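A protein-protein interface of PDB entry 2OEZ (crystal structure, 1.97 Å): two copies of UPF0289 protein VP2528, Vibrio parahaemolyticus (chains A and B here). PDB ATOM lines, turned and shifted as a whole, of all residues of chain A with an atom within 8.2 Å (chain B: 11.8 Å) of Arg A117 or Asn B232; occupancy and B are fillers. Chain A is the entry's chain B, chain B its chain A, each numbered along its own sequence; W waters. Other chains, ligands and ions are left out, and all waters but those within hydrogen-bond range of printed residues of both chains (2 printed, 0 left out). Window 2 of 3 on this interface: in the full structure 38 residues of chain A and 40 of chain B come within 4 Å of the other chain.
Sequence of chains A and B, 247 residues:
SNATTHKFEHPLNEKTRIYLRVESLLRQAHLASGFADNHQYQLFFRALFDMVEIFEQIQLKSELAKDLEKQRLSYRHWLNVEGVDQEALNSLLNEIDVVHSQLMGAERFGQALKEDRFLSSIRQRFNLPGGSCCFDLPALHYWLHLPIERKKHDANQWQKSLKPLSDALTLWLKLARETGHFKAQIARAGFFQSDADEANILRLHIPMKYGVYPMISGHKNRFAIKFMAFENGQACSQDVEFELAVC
Water W1 bridges OH of Tyr B213 and NH2 of Arg A117.
Water W2 lies within hydrogen-bond range of NE of Arg A117 (2.9 Å), O of Phe B230 (3.0 Å) and O of Glu B231 (3.3 Å).
Arg A117 touches Glu B231 (NE to O, 3.6 Å).
Asn B232 touches Arg A117 (C to CD, 3.7 Å).
CZ of Arg A117 touches N of Gly B233 (3.6 Å).
Phe A118 touches Phe B230.
Ala A139 touches Tyr B213.
Ala A139 touches Phe B230 (O to CE1, 3.3 Å).
Gly B211 touches Tyr A142 (CA to OH, 3.2 Å).
Tyr A142 touches Val B212.
Tyr A142 touches Tyr B213 (CB to CB, 3.96 Å).
Tyr A142 touches Phe B230 (CD2 to CD1, 3.4 Å).
Hydrophobic or aromatic side chains of chain B within 4 Å of the printed part of chain A: Tyr B213 and Phe B230.
Of the 16 printed residues of chain A, 4 touch a printed residue of chain B.
The backbone carbonyl oxygen of Arg A117 lies within hydrogen-bond range of the side-chain hydroxyl of Ser A120, at 3.4 Å.
N of Phe B230 sits at hydrogen-bond distance from O of Gly B211 (2.9 Å).
The backbone NH (N) of Phe A118 lies within hydrogen-bond range of the side-chain carboxylate (OD2) of Asp A116, at 3.2 Å.
The backbone carbonyl oxygen of Tyr B213 lies within hydrogen-bond range of the backbone NH of Met B228, 2.9 Å away.
The side-chain amide oxygen (OD1) of Asn B232 is in hydrogen-bond range of the backbone NH (N) of Gln B234, at 2.9 Å.
The backbone carbonyl oxygen (O) of Phe A118 lies within hydrogen-bond range of the side-chain hydroxyl (OG) of Ser A121, 2.6 Å away.
No position is printed for both chains.
Of the 11 pairs that touch across the chains among the printed residues, none has its exchanged pair printed and touching as well.
No residue of chain B comes within 4 Å of Asp A116.
Of the printed residues of chain B, Arg A117 touches Phe B230, Glu B231, Asn B232 and Gly B233.
Of chain B, only Phe B230 comes within 4 Å of Phe A118.
No residue of chain B comes within 4 Å of Leu A119.
No residue of chain B comes within 4 Å of Ser A120.
No residue of chain B comes within 4 Å of Ser A121.
Ala A139 touches two residues of chain B.
Trp A158 touches none of the printed residues of chain B.
Printed residues of chain A within 4 Å of Tyr B213: Ala A139 (3.7 Å) and Tyr A142 (3.96 Å).
Lys B226 touches none of the printed residues of chain A.
Of the printed residues of chain A, Glu B231 touches Arg A117.
Asn B232 touches one residue of chain A.
Printed residues of chain A within 4 Å of Gly B233: Arg A117 (3.6 Å).
The nearest printed residue of chain B that does not touch Arg A117 is Tyr B213 (4.8 Å).
The nearest printed residue of chain A that does not touch Glu B231 is Tyr A142 (6.5 Å).
The guanidinium group (NH2) of Arg A117 is in hydrogen-bond range of the backbone carbonyl oxygen (O) of Phe B230, at 3.0 Å.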
ATOM      1  N   ALA A 112      -6.941  23.676  -8.105  1.00  0.00           N
ATOM      2  CA  ALA A 112      -7.425  24.096  -9.429  1.00  0.00           C
ATOM      3  C   ALA A 112      -7.143  23.006 -10.458  1.00  0.00           C
ATOM      4  O   ALA A 112      -7.948  22.763 -11.308  1.00  0.00           O
ATOM      5  CB  ALA A 112      -6.818  25.409  -9.859  1.00  0.00           C
ATOM      6  N   LEU A 113      -5.990  22.349 -10.372  1.00  0.00           N
ATOM      7  CA  LEU A 113      -5.692  21.249 -11.281  1.00  0.00           C
ATOM      8  C   LEU A 113      -6.626  20.074 -11.086  1.00  0.00           C
ATOM      9  O   LEU A 113      -7.017  19.436 -12.047  1.00  0.00           O
ATOM     10  CB  LEU A 113      -4.221  20.787 -11.106  1.00  0.00           C
ATOM     11  CG  LEU A 113      -3.226  21.965 -11.300  1.00  0.00           C
ATOM     12  CD1 LEU A 113      -1.785  21.507 -10.995  1.00  0.00           C
ATOM     13  CD2 LEU A 113      -3.317  22.584 -12.768  1.00  0.00           C
ATOM     14  N   LYS A 114      -6.916  19.747  -9.834  1.00  0.00           N
ATOM     15  CA  LYS A 114      -7.863  18.671  -9.500  1.00  0.00           C
ATOM     16  C   LYS A 114      -9.304  18.945  -9.970  1.00  0.00           C
ATOM     17  O   LYS A 114      -9.983  18.033 -10.411  1.00  0.00           O
ATOM     18  CB  LYS A 114      -7.819  18.379  -8.000  1.00  0.00           C
ATOM     19  CG  LYS A 114      -6.515  17.741  -7.590  1.00  0.00           C
ATOM     20  CD  LYS A 114      -6.443  17.471  -6.101  1.00  0.00           C
ATOM     21  CE  LYS A 114      -7.335  16.299  -5.738  1.00  0.00           C
ATOM     22  NZ  LYS A 114      -7.647  16.299  -4.276  1.00  0.00           N
ATOM     23  N   GLU A 115      -9.731  20.205  -9.893  1.00  0.00           N
ATOM     24  CA  GLU A 115     -11.052  20.631 -10.316  1.00  0.00           C
ATOM     25  C   GLU A 115     -11.195  20.853 -11.825  1.00  0.00           C
ATOM     26  O   GLU A 115     -12.287  21.240 -12.294  1.00  0.00           O
ATOM     27  CB  GLU A 115     -11.414  21.947  -9.630  1.00  0.00           C
ATOM     28  CG  GLU A 115     -11.566  21.811  -8.125  1.00  0.00           C
ATOM     29  CD  GLU A 115     -12.000  23.094  -7.472  1.00  0.00           C
ATOM     30  OE1 GLU A 115     -12.113  24.126  -8.198  1.00  0.00           O
ATOM     31  OE2 GLU A 115     -12.216  23.076  -6.229  1.00  0.00           O
ATOM     32  N   ASP A 116     -10.102  20.705 -12.577  1.00  0.00           N
ATOM     33  CA  ASP A 116     -10.163  20.890 -14.024  1.00  0.00           C
ATOM     34  C   ASP A 116     -10.790  19.658 -14.655  1.00  0.00           C
ATOM     35  O   ASP A 116     -10.325  18.537 -14.432  1.00  0.00           O
ATOM     36  CB  ASP A 116      -8.758  21.161 -14.602  1.00  0.00           C
ATOM     37  CG  ASP A 116      -8.797  21.519 -16.077  1.00  0.00           C
ATOM     38  OD1 ASP A 116      -8.690  22.689 -16.389  1.00  0.00           O
ATOM     39  OD2 ASP A 116      -8.949  20.638 -16.925  1.00  0.00           O
ATOM     40  N   ARG A 117     -11.878  19.847 -15.410  1.00  0.00           N
ATOM     41  CA  ARG A 117     -12.567  18.693 -15.939  1.00  0.00           C
ATOM     42  C   ARG A 117     -11.646  17.835 -16.800  1.00  0.00           C
ATOM     43  O   ARG A 117     -11.519  16.637 -16.551  1.00  0.00           O
ATOM     44  CB  ARG A 117     -13.875  19.052 -16.693  1.00  0.00           C
ATOM     45  CG  ARG A 117     -14.653  17.764 -17.090  1.00  0.00           C
ATOM     46  CD  ARG A 117     -15.488  17.932 -18.369  1.00  0.00           C
ATOM     47  NE  ARG A 117     -14.658  17.827 -19.571  1.00  0.00           N
ATOM     48  CZ  ARG A 117     -14.178  16.674 -20.033  1.00  0.00           C
ATOM     49  NH1 ARG A 117     -14.410  15.535 -19.364  1.00  0.00           N
ATOM     50  NH2 ARG A 117     -13.419  16.660 -21.136  1.00  0.00           N
ATOM     51  N   PHE A 118     -11.024  18.435 -17.809  1.00  0.00           N
ATOM     52  CA  PHE A 118     -10.138  17.703 -18.725  1.00  0.00           C
ATOM     53  C   PHE A 118      -8.978  17.011 -17.941  1.00  0.00           C
ATOM     54  O   PHE A 118      -8.765  15.771 -18.067  1.00  0.00           O
ATOM     55  CB  PHE A 118      -9.601  18.683 -19.804  1.00  0.00           C
ATOM     56  CG  PHE A 118      -8.471  18.114 -20.634  1.00  0.00           C
ATOM     57  CD1 PHE A 118      -8.667  16.974 -21.430  1.00  0.00           C
ATOM     58  CD2 PHE A 118      -7.207  18.708 -20.599  1.00  0.00           C
ATOM     59  CE1 PHE A 118      -7.633  16.460 -22.162  1.00  0.00           C
ATOM     60  CE2 PHE A 118      -6.159  18.202 -21.339  1.00  0.00           C
ATOM     61  CZ  PHE A 118      -6.372  17.094 -22.146  1.00  0.00           C
ATOM     62  N   LEU A 119      -8.255  17.774 -17.098  1.00  0.00           N
ATOM     63  CA  LEU A 119      -7.175  17.142 -16.335  1.00  0.00           C
ATOM     64  C   LEU A 119      -7.596  15.971 -15.516  1.00  0.00           C
ATOM     65  O   LEU A 119      -6.965  14.934 -15.575  1.00  0.00           O
ATOM     66  CB  LEU A 119      -6.416  18.125 -15.441  1.00  0.00           C
ATOM     67  CG  LEU A 119      -5.650  19.194 -16.205  1.00  0.00           C
ATOM     68  CD1 LEU A 119      -4.995  20.036 -15.145  1.00  0.00           C
ATOM     69  CD2 LEU A 119      -4.647  18.642 -17.182  1.00  0.00           C
ATOM     70  N   SER A 120      -8.655  16.102 -14.732  1.00  0.00           N
ATOM     71  CA  SER A 120      -9.016  14.965 -13.898  1.00  0.00           C
ATOM     72  C   SER A 120      -9.578  13.825 -14.702  1.00  0.00           C
ATOM     73  O   SER A 120      -9.487  12.685 -14.270  1.00  0.00           O
ATOM     74  CB  SER A 120      -9.950  15.359 -12.756  1.00  0.00           C
ATOM     75  OG  SER A 120     -11.087  16.059 -13.239  1.00  0.00           O
ATOM     76  N   SER A 121     -10.098  14.082 -15.894  1.00  0.00           N
ATOM     77  CA  SER A 121     -10.542  12.959 -16.727  1.00  0.00           C
ATOM     78  C   SER A 121      -9.413  12.100 -17.310  1.00  0.00           C
ATOM     79  O   SER A 121      -9.639  10.961 -17.635  1.00  0.00           O
ATOM     80  CB  SER A 121     -11.392  13.461 -17.875  1.00  0.00           C
ATOM     81  OG  SER A 121     -10.581  14.038 -18.883  1.00  0.00           O
ATOM     82  N   ILE A 122      -8.215  12.651 -17.478  1.00  0.00           N
ATOM     83  CA  ILE A 122      -7.087  11.898 -18.015  1.00  0.00           C
ATOM     84  C   ILE A 122      -6.084  11.504 -16.947  1.00  0.00           C
ATOM     85  O   ILE A 122      -5.158  10.746 -17.231  1.00  0.00           O
ATOM     86  CB  ILE A 122      -6.335  12.651 -19.183  1.00  0.00           C
ATOM     87  CG1 ILE A 122      -5.538  13.884 -18.678  1.00  0.00           C
ATOM     88  CG2 ILE A 122      -7.306  12.947 -20.315  1.00  0.00           C
ATOM     89  CD1 ILE A 122      -4.622  14.564 -19.708  1.00  0.00           C
ATOM     90  N   ARG A 123      -6.256  12.014 -15.725  1.00  0.00           N
ATOM     91  CA  ARG A 123      -5.252  11.821 -14.653  1.00  0.00           C
ATOM     92  C   ARG A 123      -4.903  10.358 -14.301  1.00  0.00           C
ATOM     93  O   ARG A 123      -3.712   9.999 -14.221  1.00  0.00           O
ATOM     94  CB  ARG A 123      -5.672  12.578 -13.403  1.00  0.00           C
ATOM     95  CG  ARG A 123      -4.800  12.330 -12.190  1.00  0.00           C
ATOM     96  CD  ARG A 123      -4.819  13.491 -11.206  1.00  0.00           C
ATOM     97  NE  ARG A 123      -3.941  13.168 -10.081  1.00  0.00           N
ATOM     98  CZ  ARG A 123      -4.348  12.979  -8.833  1.00  0.00           C
ATOM     99  NH1 ARG A 123      -5.625  13.145  -8.522  1.00  0.00           N
ATOM    100  NH2 ARG A 123      -3.459  12.669  -7.883  1.00  0.00           N
ATOM    101  N   ALA A 139      -9.340  11.918 -25.548  1.00  0.00           N
ATOM    102  CA  ALA A 139      -9.528  13.322 -25.164  1.00  0.00           C
ATOM    103  C   ALA A 139      -8.235  14.097 -25.212  1.00  0.00           C
ATOM    104  O   ALA A 139      -8.233  15.292 -25.577  1.00  0.00           O
ATOM    105  CB  ALA A 139     -10.111  13.464 -23.793  1.00  0.00           C
ATOM    106  N   LEU A 140      -7.158  13.473 -24.721  1.00  0.00           N
ATOM    107  CA  LEU A 140      -5.819  14.051 -24.776  1.00  0.00           C
ATOM    108  C   LEU A 140      -5.396  14.204 -26.243  1.00  0.00           C
ATOM    109  O   LEU A 140      -4.916  15.256 -26.664  1.00  0.00           O
ATOM    110  CB  LEU A 140      -4.799  13.232 -23.943  1.00  0.00           C
ATOM    111  CG  LEU A 140      -3.305  13.648 -24.059  1.00  0.00           C
ATOM    112  CD1 LEU A 140      -3.092  15.119 -23.707  1.00  0.00           C
ATOM    113  CD2 LEU A 140      -2.356  12.789 -23.205  1.00  0.00           C
ATOM    114  N   TYR A 142      -7.219  14.686 -28.819  1.00  0.00           N
ATOM    115  CA  TYR A 142      -8.003  15.773 -29.418  1.00  0.00           C
ATOM    116  C   TYR A 142      -7.341  17.075 -28.969  1.00  0.00           C
ATOM    117  O   TYR A 142      -7.143  18.033 -29.715  1.00  0.00           O
ATOM    118  CB  TYR A 142      -9.447  15.682 -28.851  1.00  0.00           C
ATOM    119  CG  TYR A 142     -10.311  16.870 -29.140  1.00  0.00           C
ATOM    120  CD1 TYR A 142     -11.193  16.865 -30.249  1.00  0.00           C
ATOM    121  CD2 TYR A 142     -10.239  18.029 -28.347  1.00  0.00           C
ATOM    122  CE1 TYR A 142     -11.972  17.954 -30.511  1.00  0.00           C
ATOM    123  CE2 TYR A 142     -11.044  19.119 -28.611  1.00  0.00           C
ATOM    124  CZ  TYR A 142     -11.905  19.067 -29.691  1.00  0.00           C
ATOM    125  OH  TYR A 142     -12.690  20.194 -29.975  1.00  0.00           O
ATOM    126  N   TRP A 158      -2.874  26.568 -16.199  1.00  0.00           N
ATOM    127  CA  TRP A 158      -2.571  25.508 -15.229  1.00  0.00           C
ATOM    128  C   TRP A 158      -1.316  25.844 -14.446  1.00  0.00           C
ATOM    129  O   TRP A 158      -1.258  25.634 -13.254  1.00  0.00           O
ATOM    130  CB  TRP A 158      -2.403  24.163 -15.955  1.00  0.00           C
ATOM    131  CG  TRP A 158      -3.683  23.623 -16.568  1.00  0.00           C
ATOM    132  CD1 TRP A 158      -4.948  23.774 -16.066  1.00  0.00           C
ATOM    133  CD2 TRP A 158      -3.831  22.909 -17.816  1.00  0.00           C
ATOM    134  NE1 TRP A 158      -5.858  23.170 -16.894  1.00  0.00           N
ATOM    135  CE2 TRP A 158      -5.205  22.613 -17.965  1.00  0.00           C
ATOM    136  CE3 TRP A 158      -2.930  22.471 -18.809  1.00  0.00           C
ATOM    137  CZ2 TRP A 158      -5.711  21.917 -19.077  1.00  0.00           C
ATOM    138  CZ3 TRP A 158      -3.442  21.740 -19.926  1.00  0.00           C
ATOM    139  CH2 TRP A 158      -4.824  21.478 -20.026  1.00  0.00           C
ATOM    140  N   TYR B 210     -16.859  19.783 -34.968  1.00  0.00           N
ATOM    141  CA  TYR B 210     -17.780  19.069 -34.085  1.00  0.00           C
ATOM    142  C   TYR B 210     -17.422  19.170 -32.606  1.00  0.00           C
ATOM    143  O   TYR B 210     -18.305  19.067 -31.779  1.00  0.00           O
ATOM    144  CB  TYR B 210     -17.843  17.630 -34.480  1.00  0.00           C
ATOM    145  CG  TYR B 210     -18.535  17.375 -35.795  1.00  0.00           C
ATOM    146  CD1 TYR B 210     -19.873  17.728 -35.978  1.00  0.00           C
ATOM    147  CD2 TYR B 210     -17.869  16.758 -36.833  1.00  0.00           C
ATOM    148  CE1 TYR B 210     -20.564  17.447 -37.178  1.00  0.00           C
ATOM    149  CE2 TYR B 210     -18.548  16.462 -38.042  1.00  0.00           C
ATOM    150  CZ  TYR B 210     -19.854  16.853 -38.196  1.00  0.00           C
ATOM    151  OH  TYR B 210     -20.529  16.539 -39.346  1.00  0.00           O
ATOM    152  N   GLY B 211     -16.141  19.377 -32.296  1.00  0.00           N
ATOM    153  CA  GLY B 211     -15.680  19.508 -30.917  1.00  0.00           C
ATOM    154  C   GLY B 211     -15.788  18.164 -30.193  1.00  0.00           C
ATOM    155  O   GLY B 211     -16.065  18.109 -28.992  1.00  0.00           O
ATOM    156  N   VAL B 212     -15.607  17.092 -30.943  1.00  0.00           N
ATOM    157  CA  VAL B 212     -15.741  15.724 -30.418  1.00  0.00           C
ATOM    158  C   VAL B 212     -14.502  14.830 -30.591  1.00  0.00           C
ATOM    159  O   VAL B 212     -13.658  15.015 -31.502  1.00  0.00           O
ATOM    160  CB  VAL B 212     -16.973  14.942 -31.054  1.00  0.00           C
ATOM    161  CG1 VAL B 212     -18.271  15.599 -30.783  1.00  0.00           C
ATOM    162  CG2 VAL B 212     -16.729  14.568 -32.545  1.00  0.00           C
ATOM    163  N   TYR B 213     -14.381  13.846 -29.689  1.00  0.00           N
ATOM    164  CA  TYR B 213     -13.383  12.793 -29.792  1.00  0.00           C
ATOM    165  C   TYR B 213     -14.104  11.445 -29.695  1.00  0.00           C
ATOM    166  O   TYR B 213     -15.157  11.349 -29.145  1.00  0.00           O
ATOM    167  CB  TYR B 213     -12.243  12.878 -28.728  1.00  0.00           C
ATOM    168  CG  TYR B 213     -12.768  12.777 -27.313  1.00  0.00           C
ATOM    169  CD1 TYR B 213     -13.162  13.915 -26.643  1.00  0.00           C
ATOM    170  CD2 TYR B 213     -12.884  11.548 -26.665  1.00  0.00           C
ATOM    171  CE1 TYR B 213     -13.667  13.843 -25.382  1.00  0.00           C
ATOM    172  CE2 TYR B 213     -13.433  11.447 -25.424  1.00  0.00           C
ATOM    173  CZ  TYR B 213     -13.759  12.599 -24.764  1.00  0.00           C
ATOM    174  OH  TYR B 213     -14.293  12.542 -23.521  1.00  0.00           O
ATOM    175  N   PRO B 214     -13.533  10.407 -30.318  1.00  0.00           N
ATOM    176  CA  PRO B 214     -14.227   9.112 -30.368  1.00  0.00           C
ATOM    177  C   PRO B 214     -13.880   8.232 -29.157  1.00  0.00           C
ATOM    178  O   PRO B 214     -12.740   8.198 -28.749  1.00  0.00           O
ATOM    179  CB  PRO B 214     -13.653   8.457 -31.625  1.00  0.00           C
ATOM    180  CG  PRO B 214     -12.249   9.044 -31.741  1.00  0.00           C
ATOM    181  CD  PRO B 214     -12.227  10.397 -30.988  1.00  0.00           C
ATOM    182  N   MET B 215     -14.898   7.562 -28.631  1.00  0.00           N
ATOM    183  CA  MET B 215     -14.770   6.520 -27.631  1.00  0.00           C
ATOM    184  C   MET B 215     -15.109   5.196 -28.349  1.00  0.00           C
ATOM    185  O   MET B 215     -16.257   4.966 -28.735  1.00  0.00           O
ATOM    186  CB  MET B 215     -15.702   6.826 -26.458  1.00  0.00           C
ATOM    187  CG  MET B 215     -15.140   7.950 -25.564  1.00  0.00           C
ATOM    188  SD  MET B 215     -15.975   8.119 -23.826  1.00  0.00           S
ATOM    189  CE  MET B 215     -16.686   6.278 -23.681  1.00  0.00           C
ATOM    190  N   LYS B 226     -18.392   6.030 -30.321  1.00  0.00           N
ATOM    191  CA  LYS B 226     -19.280   6.988 -29.693  1.00  0.00           C
ATOM    192  C   LYS B 226     -18.516   8.308 -29.651  1.00  0.00           C
ATOM    193  O   LYS B 226     -17.363   8.341 -29.247  1.00  0.00           O
ATOM    194  CB  LYS B 226     -19.517   6.547 -28.286  1.00  0.00           C
ATOM    195  CG  LYS B 226     -20.509   5.435 -28.181  1.00  0.00           C
ATOM    196  CD  LYS B 226     -20.413   4.847 -26.794  1.00  0.00           C
ATOM    197  CE  LYS B 226     -21.154   3.525 -26.756  1.00  0.00           C
ATOM    198  NZ  LYS B 226     -20.265   2.542 -26.184  1.00  0.00           N
ATOM    199  N   PHE B 227     -19.141   9.363 -30.127  1.00  0.00           N
ATOM    200  CA  PHE B 227     -18.486  10.692 -30.205  1.00  0.00           C
ATOM    201  C   PHE B 227     -18.873  11.491 -28.972  1.00  0.00           C
ATOM    202  O   PHE B 227     -20.051  11.623 -28.656  1.00  0.00           O
ATOM    203  CB  PHE B 227     -18.924  11.358 -31.497  1.00  0.00           C
ATOM    204  CG  PHE B 227     -18.247  10.780 -32.698  1.00  0.00           C
ATOM    205  CD1 PHE B 227     -16.893  10.994 -32.890  1.00  0.00           C
ATOM    206  CD2 PHE B 227     -18.929   9.968 -33.582  1.00  0.00           C
ATOM    207  CE1 PHE B 227     -16.226  10.474 -33.974  1.00  0.00           C
ATOM    208  CE2 PHE B 227     -18.255   9.395 -34.664  1.00  0.00           C
ATOM    209  CZ  PHE B 227     -16.910   9.674 -34.887  1.00  0.00           C
ATOM    210  N   MET B 228     -17.869  11.939 -28.236  1.00  0.00           N
ATOM    211  CA  MET B 228     -18.092  12.616 -26.976  1.00  0.00           C
ATOM    212  C   MET B 228     -17.698  14.077 -27.133  1.00  0.00           C
ATOM    213  O   MET B 228     -16.658  14.350 -27.695  1.00  0.00           O
ATOM    214  CB  MET B 228     -17.164  12.017 -25.903  1.00  0.00           C
ATOM    215  CG  MET B 228     -17.165  10.442 -25.867  1.00  0.00           C
ATOM    216  SD  MET B 228     -18.936   9.724 -25.472  1.00  0.00           S
ATOM    217  CE  MET B 228     -19.112  10.550 -23.761  1.00  0.00           C
ATOM    218  N   ALA B 229     -18.473  14.987 -26.570  1.00  0.00           N
ATOM    219  CA  ALA B 229     -18.090  16.386 -26.620  1.00  0.00           C
ATOM    220  C   ALA B 229     -16.866  16.590 -25.716  1.00  0.00           C
ATOM    221  O   ALA B 229     -16.862  16.147 -24.546  1.00  0.00           O
ATOM    222  CB  ALA B 229     -19.225  17.279 -26.224  1.00  0.00           C
ATOM    223  N   PHE B 230     -15.851  17.272 -26.256  1.00  0.00           N
ATOM    224  CA  PHE B 230     -14.724  17.707 -25.454  1.00  0.00           C
ATOM    225  C   PHE B 230     -15.079  18.631 -24.266  1.00  0.00           C
ATOM    226  O   PHE B 230     -14.431  18.522 -23.220  1.00  0.00           O
ATOM    227  CB  PHE B 230     -13.567  18.278 -26.312  1.00  0.00           C
ATOM    228  CG  PHE B 230     -12.311  18.510 -25.525  1.00  0.00           C
ATOM    229  CD1 PHE B 230     -11.444  17.462 -25.266  1.00  0.00           C
ATOM    230  CD2 PHE B 230     -12.010  19.787 -25.011  1.00  0.00           C
ATOM    231  CE1 PHE B 230     -10.294  17.678 -24.510  1.00  0.00           C
ATOM    232  CE2 PHE B 230     -10.830  20.030 -24.278  1.00  0.00           C
ATOM    233  CZ  PHE B 230     -10.001  19.001 -23.994  1.00  0.00           C
ATOM    234  N   GLU B 231     -16.115  19.461 -24.475  1.00  0.00           N
ATOM    235  CA  GLU B 231     -16.725  20.408 -23.507  1.00  0.00           C
ATOM    236  C   GLU B 231     -17.035  19.826 -22.132  1.00  0.00           C
ATOM    237  O   GLU B 231     -16.687  20.419 -21.112  1.00  0.00           O
ATOM    238  CB  GLU B 231     -18.032  21.051 -24.080  1.00  0.00           C
ATOM    239  CG  GLU B 231     -19.350  20.218 -23.861  1.00  0.00           C
ATOM    240  CD  GLU B 231     -20.629  20.802 -24.451  1.00  0.00           C
ATOM    241  OE1 GLU B 231     -21.105  21.845 -23.951  1.00  0.00           O
ATOM    242  OE2 GLU B 231     -21.213  20.185 -25.375  1.00  0.00           O
ATOM    243  N   ASN B 232     -17.695  18.672 -22.124  1.00  0.00           N
ATOM    244  CA  ASN B 232     -18.240  18.053 -20.881  1.00  0.00           C
ATOM    245  C   ASN B 232     -17.941  16.567 -20.709  1.00  0.00           C
ATOM    246  O   ASN B 232     -18.362  15.952 -19.728  1.00  0.00           O
ATOM    247  CB  ASN B 232     -19.743  18.337 -20.700  1.00  0.00           C
ATOM    248  CG  ASN B 232     -20.605  17.757 -21.832  1.00  0.00           C
ATOM    249  OD1 ASN B 232     -20.134  17.083 -22.716  1.00  0.00           O
ATOM    250  ND2 ASN B 232     -21.869  18.017 -21.767  1.00  0.00           N
ATOM    251  N   GLY B 233     -17.258  15.994 -21.691  1.00  0.00           N
ATOM    252  CA  GLY B 233     -16.976  14.566 -21.708  1.00  0.00           C
ATOM    253  C   GLY B 233     -18.232  13.739 -21.917  1.00  0.00           C
ATOM    254  O   GLY B 233     -18.172  12.522 -21.865  1.00  0.00           O
ATOM    255  N   GLN B 234     -19.365  14.391 -22.164  1.00  0.00           N
ATOM    256  CA  GLN B 234     -20.656  13.675 -22.391  1.00  0.00           C
ATOM    257  C   GLN B 234     -20.932  13.350 -23.861  1.00  0.00           C
ATOM    258  O   GLN B 234     -20.389  13.974 -24.748  1.00  0.00           O
ATOM    259  CB  GLN B 234     -21.813  14.500 -21.825  1.00  0.00           C
ATOM    260  CG  GLN B 234     -22.583  13.912 -20.635  1.00  0.00           C
ATOM    261  CD  GLN B 234     -21.710  13.361 -19.503  1.00  0.00           C
ATOM    262  OE1 GLN B 234     -21.948  13.670 -18.341  1.00  0.00           O
ATOM    263  NE2 GLN B 234     -20.749  12.497 -19.832  1.00  0.00           N
ATOM    264  N   ALA B 235     -21.805  12.377 -24.118  1.00  0.00           N
ATOM    265  CA  ALA B 235     -22.119  11.985 -25.499  1.00  0.00           C
ATOM    266  C   ALA B 235     -22.624  13.160 -26.329  1.00  0.00           C
ATOM    267  O   ALA B 235     -23.419  13.967 -25.858  1.00  0.00           O
ATOM    268  CB  ALA B 235     -23.143  10.872 -25.512  1.00  0.00           C
ATOM    269  N   CYS B 236     -22.155  13.251 -27.567  1.00  0.00           N
ATOM    270  CA  CYS B 236     -22.608  14.278 -28.495  1.00  0.00           C
ATOM    271  C   CYS B 236     -23.780  13.725 -29.294  1.00  0.00           C
ATOM    272  O   CYS B 236     -23.666  12.680 -29.939  1.00  0.00           O
ATOM    273  CB  CYS B 236     -21.515  14.651 -29.476  1.00  0.00           C
ATOM    274  SG  CYS B 236     -21.780  13.961 -31.146  1.00  0.00           S
ATOM    275  N   SER B 237     -24.893  14.435 -29.277  1.00  0.00           N
ATOM    276  CA  SER B 237     -26.105  13.931 -29.928  1.00  0.00           C
ATOM    277  C   SER B 237     -26.214  14.292 -31.410  1.00  0.00           C
ATOM    278  O   SER B 237     -27.113  13.815 -32.102  1.00  0.00           O
ATOM    279  CB  SER B 237     -27.353  14.424 -29.171  1.00  0.00           C
ATOM    280  OG  SER B 237     -27.356  15.835 -29.046  1.00  0.00           O
ATOM    281  N   GLN B 238     -25.306  15.134 -31.892  1.00  0.00           N
ATOM    282  CA  GLN B 238     -25.333  15.642 -33.256  1.00  0.00           C
ATOM    283  C   GLN B 238     -24.944  14.494 -34.182  1.00  0.00           C
ATOM    284  O   GLN B 238     -24.283  13.536 -33.737  1.00  0.00           O
ATOM    285  CB  GLN B 238     -24.278  16.739 -33.386  1.00  0.00           C
ATOM    286  CG  GLN B 238     -24.767  18.031 -34.012  1.00  0.00           C
ATOM    287  CD  GLN B 238     -23.649  18.794 -34.753  1.00  0.00           C
ATOM    288  OE1 GLN B 238     -22.578  19.129 -34.175  1.00  0.00           O
ATOM    289  NE2 GLN B 238     -23.899  19.071 -36.043  1.00  0.00           N
HETATM  290  O   HOH W   1     -13.147  13.977 -21.593  1.00  0.00           O
HETATM  291  O   HOH W   2     -13.390  20.096 -20.867  1.00  0.00           O
